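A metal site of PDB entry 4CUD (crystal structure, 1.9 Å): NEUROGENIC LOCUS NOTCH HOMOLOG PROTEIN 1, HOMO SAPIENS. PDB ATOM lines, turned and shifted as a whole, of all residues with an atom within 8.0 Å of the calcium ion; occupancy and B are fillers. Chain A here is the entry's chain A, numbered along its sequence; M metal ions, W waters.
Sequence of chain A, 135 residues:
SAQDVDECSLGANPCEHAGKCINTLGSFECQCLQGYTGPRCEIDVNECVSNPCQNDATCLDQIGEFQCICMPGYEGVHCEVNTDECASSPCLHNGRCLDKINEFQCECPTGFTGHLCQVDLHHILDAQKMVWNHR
The backbone NH (N) of Gly 26 sits close to the side-chain carboxylate (OD1) of Asp 4, at 2.8 Å.
The side-chain hydroxyl of Thr 24 sits close to the backbone NH of Ser 27 (3.3 Å).
The side-chain hydroxyl of Thr 24 lies within hydrogen-bond range of the backbone NH of Phe 28 (3.4 Å).
The side-chain sulfur (SG) of Cys 8 sits at hydrogen-bond distance from the backbone NH (N) of Asn 23 (3.3 Å).
Gly 26 touches the calcium ion.
Seven residues have an atom within 4 Å of the calcium ion: Asp 4, Val 5, Glu 7, Asn 23, Thr 24, Gly 26 and Ser 27.
The side-chain amide oxygen (OD1) of Asn 23 is bound to the calcium ion, 2.3 Å away.
The backbone carbonyl oxygen (O) of Thr 24 binds the calcium ion, 2.4 Å away.
The calcium ion is bound by O of Ser 27.
The calcium ion is bound by OE1 of Glu 7 (2.4 Å).
The calcium ion is bound by water W1 (2.5 Å).
O of Val 5 binds the calcium ion, at 2.5 Å.
The side-chain carboxylate (OD1) of Asp 4 is bound to the calcium ion (2.6 Å).
Slightly farther from the calcium ion lies OD2 of Asp 4 (3.1 Å).
Water W1 lies within hydrogen-bond range of OE2 of Glu 7 (2.6 Å), N of Ser 27 (3.0 Å) and O of Gly 26 (3.2 Å).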
ATOM      1  N   ASP A   4      -4.119  18.617   2.922  1.00  0.00           N
ATOM      2  CA  ASP A   4      -5.331  18.415   3.778  1.00  0.00           C
ATOM      3  C   ASP A   4      -5.195  17.209   4.717  1.00  0.00           C
ATOM      4  O   ASP A   4      -4.663  16.163   4.339  1.00  0.00           O
ATOM      5  CB  ASP A   4      -6.575  18.234   2.901  1.00  0.00           C
ATOM      6  CG  ASP A   4      -7.849  18.050   3.720  1.00  0.00           C
ATOM      7  OD1 ASP A   4      -8.150  18.927   4.550  1.00  0.00           O
ATOM      8  OD2 ASP A   4      -8.541  17.027   3.533  1.00  0.00           O
ATOM      9  N   VAL A   5      -5.668  17.388   5.946  1.00  0.00           N
ATOM     10  CA  VAL A   5      -5.835  16.287   6.898  1.00  0.00           C
ATOM     11  C   VAL A   5      -7.298  15.839   6.827  1.00  0.00           C
ATOM     12  O   VAL A   5      -8.214  16.663   6.860  1.00  0.00           O
ATOM     13  CB  VAL A   5      -5.472  16.737   8.343  1.00  0.00           C
ATOM     14  CG1 VAL A   5      -6.141  15.877   9.392  1.00  0.00           C
ATOM     15  CG2 VAL A   5      -3.956  16.730   8.531  1.00  0.00           C
ATOM     16  N   ASP A   6      -7.519  14.533   6.684  1.00  0.00           N
ATOM     17  CA  ASP A   6      -8.854  13.974   6.811  1.00  0.00           C
ATOM     18  C   ASP A   6      -9.209  13.814   8.299  1.00  0.00           C
ATOM     19  O   ASP A   6      -8.825  12.840   8.934  1.00  0.00           O
ATOM     20  CB  ASP A   6      -8.943  12.616   6.089  1.00  0.00           C
ATOM     21  CG  ASP A   6     -10.354  12.031   6.087  1.00  0.00           C
ATOM     22  OD1 ASP A   6     -11.250  12.568   6.784  1.00  0.00           O
ATOM     23  OD2 ASP A   6     -10.582  11.036   5.373  1.00  0.00           O
ATOM     24  N   GLU A   7      -9.966  14.771   8.839  1.00  0.00           N
ATOM     25  CA  GLU A   7     -10.348  14.717  10.244  1.00  0.00           C
ATOM     26  C   GLU A   7     -11.290  13.563  10.571  1.00  0.00           C
ATOM     27  O   GLU A   7     -11.465  13.235  11.739  1.00  0.00           O
ATOM     28  CB  GLU A   7     -10.939  16.042  10.752  1.00  0.00           C
ATOM     29  CG  GLU A   7      -9.977  17.223  10.751  1.00  0.00           C
ATOM     30  CD  GLU A   7     -10.008  18.018   9.452  1.00  0.00           C
ATOM     31  OE1 GLU A   7     -10.384  17.457   8.389  1.00  0.00           O
ATOM     32  OE2 GLU A   7      -9.658  19.217   9.479  1.00  0.00           O
ATOM     33  N   CYS A   8     -11.895  12.967   9.546  1.00  0.00           N
ATOM     34  CA  CYS A   8     -12.780  11.794   9.721  1.00  0.00           C
ATOM     35  C   CYS A   8     -12.031  10.452   9.685  1.00  0.00           C
ATOM     36  O   CYS A   8     -12.660   9.400   9.736  1.00  0.00           O
ATOM     37  CB  CYS A   8     -13.866  11.772   8.656  1.00  0.00           C
ATOM     38  SG  CYS A   8     -14.720  13.336   8.489  1.00  0.00           S
ATOM     39  N   ILE A  22     -17.853  14.106   7.770  1.00  0.00           N
ATOM     40  CA  ILE A  22     -17.608  14.340   6.347  1.00  0.00           C
ATOM     41  C   ILE A  22     -16.377  15.218   6.168  1.00  0.00           C
ATOM     42  O   ILE A  22     -16.349  16.372   6.606  1.00  0.00           O
ATOM     43  CB  ILE A  22     -18.841  14.981   5.674  1.00  0.00           C
ATOM     44  CG1 ILE A  22     -20.016  13.991   5.639  1.00  0.00           C
ATOM     45  CG2 ILE A  22     -18.491  15.465   4.264  1.00  0.00           C
ATOM     46  CD1 ILE A  22     -21.369  14.614   5.374  1.00  0.00           C
ATOM     47  N   ASN A  23     -15.348  14.673   5.517  1.00  0.00           N
ATOM     48  CA  ASN A  23     -14.123  15.447   5.267  1.00  0.00           C
ATOM     49  C   ASN A  23     -14.310  16.537   4.213  1.00  0.00           C
ATOM     50  O   ASN A  23     -14.977  16.322   3.192  1.00  0.00           O
ATOM     51  CB  ASN A  23     -12.954  14.532   4.875  1.00  0.00           C
ATOM     52  CG  ASN A  23     -11.635  15.283   4.770  1.00  0.00           C
ATOM     53  OD1 ASN A  23     -11.341  16.172   5.579  1.00  0.00           O
ATOM     54  ND2 ASN A  23     -10.828  14.942   3.773  1.00  0.00           N
ATOM     55  N   THR A  24     -13.715  17.694   4.465  1.00  0.00           N
ATOM     56  CA  THR A  24     -13.589  18.742   3.435  1.00  0.00           C
ATOM     57  C   THR A  24     -12.127  19.159   3.306  1.00  0.00           C
ATOM     58  O   THR A  24     -11.279  18.791   4.128  1.00  0.00           O
ATOM     59  CB  THR A  24     -14.468  19.977   3.711  1.00  0.00           C
ATOM     60  OG1 THR A  24     -13.884  20.765   4.748  1.00  0.00           O
ATOM     61  CG2 THR A  24     -15.912  19.593   4.098  1.00  0.00           C
ATOM     62  N   LEU A  25     -11.821  19.934   2.276  1.00  0.00           N
ATOM     63  CA  LEU A  25     -10.447  20.389   2.078  1.00  0.00           C
ATOM     64  C   LEU A  25     -10.154  21.584   2.996  1.00  0.00           C
ATOM     65  O   LEU A  25     -10.656  22.679   2.763  1.00  0.00           O
ATOM     66  CB  LEU A  25     -10.184  20.710   0.596  1.00  0.00           C
ATOM     67  CG  LEU A  25     -10.544  19.592  -0.393  1.00  0.00           C
ATOM     68  CD1 LEU A  25     -10.426  20.038  -1.841  1.00  0.00           C
ATOM     69  CD2 LEU A  25      -9.717  18.334  -0.148  1.00  0.00           C
ATOM     70  N   GLY A  26      -9.375  21.359   4.048  1.00  0.00           N
ATOM     71  CA  GLY A  26      -9.074  22.416   5.014  1.00  0.00           C
ATOM     72  C   GLY A  26      -9.921  22.380   6.273  1.00  0.00           C
ATOM     73  O   GLY A  26      -9.580  22.999   7.283  1.00  0.00           O
ATOM     74  N   SER A  27     -11.048  21.659   6.224  1.00  0.00           N
ATOM     75  CA  SER A  27     -11.852  21.460   7.423  1.00  0.00           C
ATOM     76  C   SER A  27     -12.592  20.114   7.387  1.00  0.00           C
ATOM     77  O   SER A  27     -12.104  19.138   6.804  1.00  0.00           O
ATOM     78  CB  SER A  27     -12.817  22.651   7.599  1.00  0.00           C
ATOM     79  OG  SER A  27     -13.363  22.684   8.893  1.00  0.00           O
ATOM     80  N   PHE A  28     -13.745  20.051   8.039  1.00  0.00           N
ATOM     81  CA  PHE A  28     -14.653  18.896   7.967  1.00  0.00           C
ATOM     82  C   PHE A  28     -16.024  19.384   8.390  1.00  0.00           C
ATOM     83  O   PHE A  28     -16.170  20.520   8.838  1.00  0.00           O
ATOM     84  CB  PHE A  28     -14.181  17.736   8.880  1.00  0.00           C
ATOM     85  CG  PHE A  28     -14.294  18.042  10.347  1.00  0.00           C
ATOM     86  CD1 PHE A  28     -13.309  18.776  11.005  1.00  0.00           C
ATOM     87  CD2 PHE A  28     -15.397  17.622  11.080  1.00  0.00           C
ATOM     88  CE1 PHE A  28     -13.422  19.077  12.360  1.00  0.00           C
ATOM     89  CE2 PHE A  28     -15.511  17.923  12.435  1.00  0.00           C
ATOM     90  CZ  PHE A  28     -14.517  18.645  13.066  1.00  0.00           C
ATOM     91  N   GLU A  29     -17.036  18.527   8.245  1.00  0.00           N
ATOM     92  CA  GLU A  29     -18.391  18.826   8.713  1.00  0.00           C
ATOM     93  C   GLU A  29     -19.056  17.604   9.328  1.00  0.00           C
ATOM     94  O   GLU A  29     -18.694  16.462   9.018  1.00  0.00           O
ATOM     95  CB  GLU A  29     -19.245  19.419   7.570  1.00  0.00           C
ATOM     96  CG  GLU A  29     -19.559  18.453   6.439  1.00  0.00           C
ATOM     97  CD  GLU A  29     -20.105  19.146   5.191  1.00  0.00           C
ATOM     98  OE1 GLU A  29     -20.216  20.388   5.168  1.00  0.00           O
ATOM     99  OE2 GLU A  29     -20.433  18.419   4.213  1.00  0.00           O
HETATM  100 CA    CA M   1     -10.083  18.054   6.047  1.00  0.00          CA
HETATM  101  O   HOH W   1      -8.807  19.876   7.091  1.00  0.00           O
